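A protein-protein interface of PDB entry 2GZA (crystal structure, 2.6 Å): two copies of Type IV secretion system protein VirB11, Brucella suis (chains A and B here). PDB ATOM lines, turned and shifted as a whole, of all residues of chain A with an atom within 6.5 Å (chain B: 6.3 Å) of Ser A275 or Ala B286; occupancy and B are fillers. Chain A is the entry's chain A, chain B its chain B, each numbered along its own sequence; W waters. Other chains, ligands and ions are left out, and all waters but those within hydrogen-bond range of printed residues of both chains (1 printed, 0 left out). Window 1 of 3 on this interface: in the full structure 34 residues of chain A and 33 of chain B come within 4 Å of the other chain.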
ATOM      1  N   LEU A 249     -17.858  16.769   1.158  1.00  0.00           N
ATOM      2  CA  LEU A 249     -17.373  18.153   1.115  1.00  0.00           C
ATOM      3  C   LEU A 249     -18.179  19.026   0.152  1.00  0.00           C
ATOM      4  O   LEU A 249     -18.304  20.227   0.357  1.00  0.00           O
ATOM      5  CB  LEU A 249     -15.886  18.193   0.725  1.00  0.00           C
ATOM      6  CG  LEU A 249     -14.843  17.425   1.552  1.00  0.00           C
ATOM      7  CD1 LEU A 249     -13.480  17.449   0.874  1.00  0.00           C
ATOM      8  CD2 LEU A 249     -14.732  17.967   2.962  1.00  0.00           C
ATOM      9  N   ILE A 270      -9.796  12.787   9.082  1.00  0.00           N
ATOM     10  CA  ILE A 270      -9.029  13.853   9.714  1.00  0.00           C
ATOM     11  C   ILE A 270      -9.143  15.121   8.895  1.00  0.00           C
ATOM     12  O   ILE A 270      -9.415  16.195   9.435  1.00  0.00           O
ATOM     13  CB  ILE A 270      -7.546  13.429   9.889  1.00  0.00           C
ATOM     14  CG1 ILE A 270      -7.414  12.468  11.067  1.00  0.00           C
ATOM     15  CG2 ILE A 270      -6.642  14.631  10.109  1.00  0.00           C
ATOM     16  CD1 ILE A 270      -6.043  11.784  11.141  1.00  0.00           C
ATOM     17  N   ASN A 271      -8.963  14.968   7.590  1.00  0.00           N
ATOM     18  CA  ASN A 271      -8.947  16.071   6.651  1.00  0.00           C
ATOM     19  C   ASN A 271     -10.289  16.791   6.560  1.00  0.00           C
ATOM     20  O   ASN A 271     -10.342  18.016   6.508  1.00  0.00           O
ATOM     21  CB  ASN A 271      -8.555  15.534   5.282  1.00  0.00           C
ATOM     22  CG  ASN A 271      -7.709  16.503   4.499  1.00  0.00           C
ATOM     23  OD1 ASN A 271      -7.371  17.588   4.967  1.00  0.00           O
ATOM     24  ND2 ASN A 271      -7.356  16.111   3.301  1.00  0.00           N
ATOM     25  N   VAL A 272     -11.359  16.007   6.540  1.00  0.00           N
ATOM     26  CA  VAL A 272     -12.723  16.505   6.514  1.00  0.00           C
ATOM     27  C   VAL A 272     -13.046  17.269   7.808  1.00  0.00           C
ATOM     28  O   VAL A 272     -13.596  18.362   7.764  1.00  0.00           O
ATOM     29  CB  VAL A 272     -13.733  15.333   6.269  1.00  0.00           C
ATOM     30  CG1 VAL A 272     -15.169  15.769   6.509  1.00  0.00           C
ATOM     31  CG2 VAL A 272     -13.583  14.768   4.862  1.00  0.00           C
ATOM     32  N   ALA A 273     -12.679  16.693   8.947  1.00  0.00           N
ATOM     33  CA  ALA A 273     -12.904  17.313  10.248  1.00  0.00           C
ATOM     34  C   ALA A 273     -12.058  18.563  10.449  1.00  0.00           C
ATOM     35  O   ALA A 273     -12.534  19.552  11.004  1.00  0.00           O
ATOM     36  CB  ALA A 273     -12.646  16.315  11.347  1.00  0.00           C
ATOM     37  N   ALA A 274     -10.811  18.512   9.993  1.00  0.00           N
ATOM     38  CA  ALA A 274      -9.949  19.687   9.973  1.00  0.00           C
ATOM     39  C   ALA A 274     -10.528  20.801   9.084  1.00  0.00           C
ATOM     40  O   ALA A 274     -10.271  21.967   9.320  1.00  0.00           O
ATOM     41  CB  ALA A 274      -8.544  19.294   9.519  1.00  0.00           C
ATOM     42  N   SER A 275     -11.322  20.425   8.084  1.00  0.00           N
ATOM     43  CA  SER A 275     -11.932  21.380   7.130  1.00  0.00           C
ATOM     44  C   SER A 275     -13.039  22.209   7.753  1.00  0.00           C
ATOM     45  O   SER A 275     -13.515  23.174   7.158  1.00  0.00           O
ATOM     46  CB  SER A 275     -12.531  20.654   5.925  1.00  0.00           C
ATOM     47  OG  SER A 275     -11.555  19.903   5.235  1.00  0.00           O
ATOM     48  N   GLY A 276     -13.461  21.809   8.942  1.00  0.00           N
ATOM     49  CA  GLY A 276     -14.480  22.542   9.658  1.00  0.00           C
ATOM     50  C   GLY A 276     -15.750  21.749   9.857  1.00  0.00           C
ATOM     51  O   GLY A 276     -16.637  22.196  10.577  1.00  0.00           O
ATOM     52  N   HIS A 277     -15.849  20.580   9.224  1.00  0.00           N
ATOM     53  CA  HIS A 277     -17.015  19.717   9.422  1.00  0.00           C
ATOM     54  C   HIS A 277     -16.986  19.102  10.816  1.00  0.00           C
ATOM     55  O   HIS A 277     -16.276  18.121  11.058  1.00  0.00           O
ATOM     56  CB  HIS A 277     -17.096  18.629   8.348  1.00  0.00           C
ATOM     57  CG  HIS A 277     -17.474  19.150   7.000  1.00  0.00           C
ATOM     58  ND1 HIS A 277     -16.642  19.056   5.907  1.00  0.00           N
ATOM     59  CD2 HIS A 277     -18.586  19.795   6.574  1.00  0.00           C
ATOM     60  CE1 HIS A 277     -17.230  19.611   4.863  1.00  0.00           C
ATOM     61  NE2 HIS A 277     -18.410  20.068   5.242  1.00  0.00           N
ATOM     62  N   VAL A 321      -8.471  16.915  16.204  1.00  0.00           N
ATOM     63  CA  VAL A 321      -9.699  16.647  15.478  1.00  0.00           C
ATOM     64  C   VAL A 321     -10.711  15.836  16.292  1.00  0.00           C
ATOM     65  O   VAL A 321     -11.921  16.046  16.174  1.00  0.00           O
ATOM     66  CB  VAL A 321      -9.371  15.972  14.129  1.00  0.00           C
ATOM     67  CG1 VAL A 321     -10.466  15.033  13.681  1.00  0.00           C
ATOM     68  CG2 VAL A 321      -9.086  17.032  13.075  1.00  0.00           C
ATOM     69  N   ALA B 181      -9.555  31.774   6.321  1.00  0.00           N
ATOM     70  CA  ALA B 181      -9.961  30.434   6.716  1.00  0.00           C
ATOM     71  C   ALA B 181     -11.359  30.418   7.308  1.00  0.00           C
ATOM     72  O   ALA B 181     -11.867  31.438   7.770  1.00  0.00           O
ATOM     73  CB  ALA B 181      -8.967  29.836   7.702  1.00  0.00           C
ATOM     74  N   GLY B 182     -11.971  29.246   7.300  1.00  0.00           N
ATOM     75  CA  GLY B 182     -13.315  29.073   7.829  1.00  0.00           C
ATOM     76  C   GLY B 182     -13.913  27.786   7.315  1.00  0.00           C
ATOM     77  O   GLY B 182     -13.373  27.167   6.400  1.00  0.00           O
ATOM     78  N   GLU B 183     -15.026  27.359   7.897  1.00  0.00           N
ATOM     79  CA  GLU B 183     -15.704  26.202   7.335  1.00  0.00           C
ATOM     80  C   GLU B 183     -16.489  26.593   6.088  1.00  0.00           C
ATOM     81  O   GLU B 183     -16.659  27.777   5.797  1.00  0.00           O
ATOM     82  CB  GLU B 183     -16.592  25.498   8.345  1.00  0.00           C
ATOM     83  CG  GLU B 183     -17.884  26.199   8.671  1.00  0.00           C
ATOM     84  CD  GLU B 183     -18.766  25.331   9.516  1.00  0.00           C
ATOM     85  OE1 GLU B 183     -18.259  24.756  10.501  1.00  0.00           O
ATOM     86  OE2 GLU B 183     -19.957  25.209   9.177  1.00  0.00           O
ATOM     87  N   THR B 184     -16.944  25.598   5.335  1.00  0.00           N
ATOM     88  CA  THR B 184     -17.700  25.882   4.115  1.00  0.00           C
ATOM     89  C   THR B 184     -18.995  26.630   4.438  1.00  0.00           C
ATOM     90  O   THR B 184     -19.754  26.258   5.339  1.00  0.00           O
ATOM     91  CB  THR B 184     -18.030  24.626   3.242  1.00  0.00           C
ATOM     92  OG1 THR B 184     -16.913  23.738   3.195  1.00  0.00           O
ATOM     93  CG2 THR B 184     -18.363  25.034   1.808  1.00  0.00           C
ATOM     94  N   LYS B 188     -16.056  33.156   3.584  1.00  0.00           N
ATOM     95  CA  LYS B 188     -14.636  33.396   3.286  1.00  0.00           C
ATOM     96  C   LYS B 188     -14.446  34.242   2.039  1.00  0.00           C
ATOM     97  O   LYS B 188     -13.713  35.226   2.052  1.00  0.00           O
ATOM     98  CB  LYS B 188     -13.873  32.083   3.101  1.00  0.00           C
ATOM     99  CG  LYS B 188     -13.605  31.297   4.368  1.00  0.00           C
ATOM    100  CD  LYS B 188     -12.839  30.015   4.052  1.00  0.00           C
ATOM    101  CE  LYS B 188     -13.763  28.827   3.834  1.00  0.00           C
ATOM    102  NZ  LYS B 188     -14.403  28.817   2.503  1.00  0.00           N
ATOM    103  N   CYS B 284      -9.115  28.942   2.384  1.00  0.00           N
ATOM    104  CA  CYS B 284      -8.905  27.554   2.692  1.00  0.00           C
ATOM    105  C   CYS B 284      -9.948  27.114   3.708  1.00  0.00           C
ATOM    106  O   CYS B 284     -10.115  27.764   4.738  1.00  0.00           O
ATOM    107  CB  CYS B 284      -7.493  27.375   3.259  1.00  0.00           C
ATOM    108  SG  CYS B 284      -7.036  25.694   3.638  1.00  0.00           S
ATOM    109  N   HIS B 285     -10.646  26.024   3.420  1.00  0.00           N
ATOM    110  CA  HIS B 285     -11.563  25.434   4.386  1.00  0.00           C
ATOM    111  C   HIS B 285     -10.761  24.871   5.546  1.00  0.00           C
ATOM    112  O   HIS B 285      -9.935  23.979   5.346  1.00  0.00           O
ATOM    113  CB  HIS B 285     -12.388  24.317   3.751  1.00  0.00           C
ATOM    114  CG  HIS B 285     -13.201  24.758   2.581  1.00  0.00           C
ATOM    115  ND1 HIS B 285     -14.416  25.398   2.715  1.00  0.00           N
ATOM    116  CD2 HIS B 285     -12.975  24.648   1.254  1.00  0.00           C
ATOM    117  CE1 HIS B 285     -14.904  25.668   1.520  1.00  0.00           C
ATOM    118  NE2 HIS B 285     -14.047  25.225   0.617  1.00  0.00           N
ATOM    119  N   ALA B 286     -10.989  25.404   6.745  1.00  0.00           N
ATOM    120  CA  ALA B 286     -10.335  24.915   7.962  1.00  0.00           C
ATOM    121  C   ALA B 286     -11.129  25.296   9.197  1.00  0.00           C
ATOM    122  O   ALA B 286     -11.824  26.308   9.204  1.00  0.00           O
ATOM    123  CB  ALA B 286      -8.922  25.442   8.064  1.00  0.00           C
ATOM    124  N   GLY B 287     -11.008  24.483  10.244  1.00  0.00           N
ATOM    125  CA  GLY B 287     -11.753  24.666  11.489  1.00  0.00           C
ATOM    126  C   GLY B 287     -11.111  25.600  12.488  1.00  0.00           C
ATOM    127  O   GLY B 287     -11.684  25.872  13.540  1.00  0.00           O
ATOM    128  N   SER B 288      -9.913  26.075  12.165  1.00  0.00           N
ATOM    129  CA  SER B 288      -9.201  27.077  12.961  1.00  0.00           C
ATOM    130  C   SER B 288      -7.950  27.522  12.213  1.00  0.00           C
ATOM    131  O   SER B 288      -7.637  26.995  11.151  1.00  0.00           O
ATOM    132  CB  SER B 288      -8.828  26.544  14.352  1.00  0.00           C
ATOM    133  OG  SER B 288      -7.799  25.573  14.288  1.00  0.00           O
ATOM    134  N   CYS B 289      -7.244  28.497  12.773  1.00  0.00           N
ATOM    135  CA  CYS B 289      -5.989  28.967  12.193  1.00  0.00           C
ATOM    136  C   CYS B 289      -4.915  27.874  12.138  1.00  0.00           C
ATOM    137  O   CYS B 289      -4.285  27.686  11.107  1.00  0.00           O
ATOM    138  CB  CYS B 289      -5.468  30.194  12.938  1.00  0.00           C
ATOM    139  SG  CYS B 289      -6.453  31.667  12.646  1.00  0.00           S
ATOM    140  N   LEU B 291      -5.427  24.630  12.235  1.00  0.00           N
ATOM    141  CA  LEU B 291      -5.930  23.647  11.287  1.00  0.00           C
ATOM    142  C   LEU B 291      -5.736  24.074   9.832  1.00  0.00           C
ATOM    143  O   LEU B 291      -5.677  23.226   8.943  1.00  0.00           O
ATOM    144  CB  LEU B 291      -7.395  23.292  11.573  1.00  0.00           C
ATOM    145  CG  LEU B 291      -7.647  22.409  12.798  1.00  0.00           C
ATOM    146  CD1 LEU B 291      -9.123  22.388  13.167  1.00  0.00           C
ATOM    147  CD2 LEU B 291      -7.122  20.997  12.574  1.00  0.00           C
ATOM    148  N   THR B 292      -5.638  25.381   9.594  1.00  0.00           N
ATOM    149  CA  THR B 292      -5.328  25.907   8.265  1.00  0.00           C
ATOM    150  C   THR B 292      -3.936  25.441   7.843  1.00  0.00           C
ATOM    151  O   THR B 292      -3.781  24.840   6.790  1.00  0.00           O
ATOM    152  CB  THR B 292      -5.408  27.453   8.197  1.00  0.00           C
ATOM    153  OG1 THR B 292      -6.682  27.895   8.680  1.00  0.00           O
ATOM    154  CG2 THR B 292      -5.220  27.942   6.773  1.00  0.00           C
ATOM    155  N   PHE B 293      -2.928  25.697   8.670  1.00  0.00           N
ATOM    156  CA  PHE B 293      -1.573  25.246   8.351  1.00  0.00           C
ATOM    157  C   PHE B 293      -1.508  23.728   8.293  1.00  0.00           C
ATOM    158  O   PHE B 293      -0.753  23.149   7.508  1.00  0.00           O
ATOM    159  CB  PHE B 293      -0.551  25.781   9.350  1.00  0.00           C
ATOM    160  CG  PHE B 293      -0.245  27.241   9.189  1.00  0.00           C
ATOM    161  CD1 PHE B 293       0.557  27.685   8.142  1.00  0.00           C
ATOM    162  CD2 PHE B 293      -0.737  28.168  10.097  1.00  0.00           C
ATOM    163  CE1 PHE B 293       0.853  29.027   7.993  1.00  0.00           C
ATOM    164  CE2 PHE B 293      -0.445  29.512   9.959  1.00  0.00           C
ATOM    165  CZ  PHE B 293       0.350  29.943   8.903  1.00  0.00           C
ATOM    166  N   ARG B 295      -4.017  21.715   7.343  1.00  0.00           N
ATOM    167  CA  ARG B 295      -4.599  21.291   6.070  1.00  0.00           C
ATOM    168  C   ARG B 295      -3.770  21.689   4.862  1.00  0.00           C
ATOM    169  O   ARG B 295      -3.720  20.948   3.881  1.00  0.00           O
ATOM    170  CB  ARG B 295      -6.040  21.774   5.914  1.00  0.00           C
ATOM    171  CG  ARG B 295      -7.022  20.969   6.726  1.00  0.00           C
ATOM    172  CD  ARG B 295      -8.422  21.092   6.187  1.00  0.00           C
ATOM    173  NE  ARG B 295      -8.630  20.291   4.988  1.00  0.00           N
ATOM    174  CZ  ARG B 295      -9.019  20.773   3.814  1.00  0.00           C
ATOM    175  NH1 ARG B 295      -9.270  22.070   3.651  1.00  0.00           N
ATOM    176  NH2 ARG B 295      -9.178  19.946   2.800  1.00  0.00           N
ATOM    177  N   HIS B 327      -9.513  33.566  10.480  1.00  0.00           N
ATOM    178  CA  HIS B 327     -10.518  32.516  10.568  1.00  0.00           C
ATOM    179  C   HIS B 327     -11.926  33.082  10.772  1.00  0.00           C
ATOM    180  O   HIS B 327     -12.170  33.876  11.686  1.00  0.00           O
ATOM    181  CB  HIS B 327     -10.167  31.505  11.667  1.00  0.00           C
ATOM    182  CG  HIS B 327     -11.195  30.437  11.843  1.00  0.00           C
ATOM    183  ND1 HIS B 327     -11.376  29.424  10.929  1.00  0.00           N
ATOM    184  CD2 HIS B 327     -12.118  30.237  12.813  1.00  0.00           C
ATOM    185  CE1 HIS B 327     -12.360  28.644  11.331  1.00  0.00           C
ATOM    186  NE2 HIS B 327     -12.827  29.116  12.473  1.00  0.00           N
ATOM    187  N   VAL B 328     -12.845  32.668   9.909  1.00  0.00           N
ATOM    188  CA  VAL B 328     -14.244  33.087  10.004  1.00  0.00           C
ATOM    189  C   VAL B 328     -15.080  31.959  10.593  1.00  0.00           C
ATOM    190  O   VAL B 328     -14.939  30.801  10.214  1.00  0.00           O
ATOM    191  CB  VAL B 328     -14.819  33.531   8.643  1.00  0.00           C
ATOM    192  CG1 VAL B 328     -16.153  34.247   8.837  1.00  0.00           C
ATOM    193  CG2 VAL B 328     -13.853  34.438   7.937  1.00  0.00           C
HETATM  194  O   HOH W   1     -16.359  24.717  12.524  1.00  0.00           O
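The side-chain amino group (NZ) of Lys B188 lies close to a ring nitrogen (ND1) of His B285, at 3.4 Å.
O of Asn A271 lies within hydrogen-bond range of OG of Ser A275, at 2.6 Å.
OG1 of Thr B184 sits at hydrogen-bond distance from ND1 of His B285 (3.0 Å).
The side-chain hydroxyl (OG) of Ser B288 lies within hydrogen-bond range of the backbone NH (N) of Leu B291.
The backbone carbonyl oxygen (O) of His B285 sits at hydrogen-bond distance from the guanidinium group (NH1) of Arg B295, 2.6 Å away.
O of Gly B182 is in hydrogen-bond range of N of Ala B286 (3.0 Å).
Water W1 lies within hydrogen-bond range of the side-chain carboxylate (OE1) of Glu B183 (2.8 Å) and the backbone carbonyl oxygen (O) of Gly A276 (3.2 Å).
Ser A275 touches five residues of chain B.
Printed residues of chain B within 4 Å of Gly A276: Glu B183 and Gly B287.
Thr B184 touches none of the printed residues of chain A.
Cys B284 touches none of the printed residues of chain A.
Ala B286 touches two residues of chain A.
Of the printed residues of chain A, Leu B291 touches Ala A274.
The nearest residue of chain B that does not touch Ser A275 is Gly B182 (4.1 Å).
The nearest printed residue of chain A that does not touch His B285 is Ala A274 (4.5 Å).
No position is printed for both chains.
Of the 12 pairs that touch across the chains among the printed residues, none has its exchanged pair printed and touching as well.
Printed residues of chain B that touch a printed residue of chain A: Glu B183, His B285, Ala B286, Gly B287, Leu B291 and Arg B295.
Hydrophobic or aromatic side chains of chain B that line the printed part of chain A: His B285, Ala B286 and Leu B291.
Hydrophobic or aromatic side chains of chain A that line the printed part of chain B: Ala A274.
Among the printed residues, 12 pairs touch across the chains.
Among the printed residues, no Asp or Glu carboxylate lies within 4 Å of a Lys or Arg side-chain nitrogen of the other chain.
Among the printed residues, merely in contact across the chains: Ala A274 with Ala B286 (3.2 Å), Ala A274 with Arg B295 (3.6 Å), Ser A275 with His B285 (3.6 Å), Ser A275 with Glu B183 (3.7 Å), Ala A274 with Leu B291 (3.8 Å), Gly A276 with Gly B287 (3.9 Å) and Ser A275 with Gly B287 (3.9 Å).
O of Ala A274 lies within hydrogen-bond range of N of Gly B287 (2.8 Å).
The side-chain amide oxygen of Asn A271 is in hydrogen-bond range of the guanidinium group of Arg B295 (3.0 Å).
The guanidinium group (NE) of Arg B295 lies within hydrogen-bond range of the side-chain hydroxyl (OG) of Ser A275 (3.0 Å).
The backbone carbonyl oxygen of Ser A275 lies within hydrogen-bond range of the backbone NH of Ala B286.
The backbone carbonyl oxygen (O) of Gly A276 lies close to the side-chain carboxylate (OE1) of Glu B183, at 3.0 Å.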
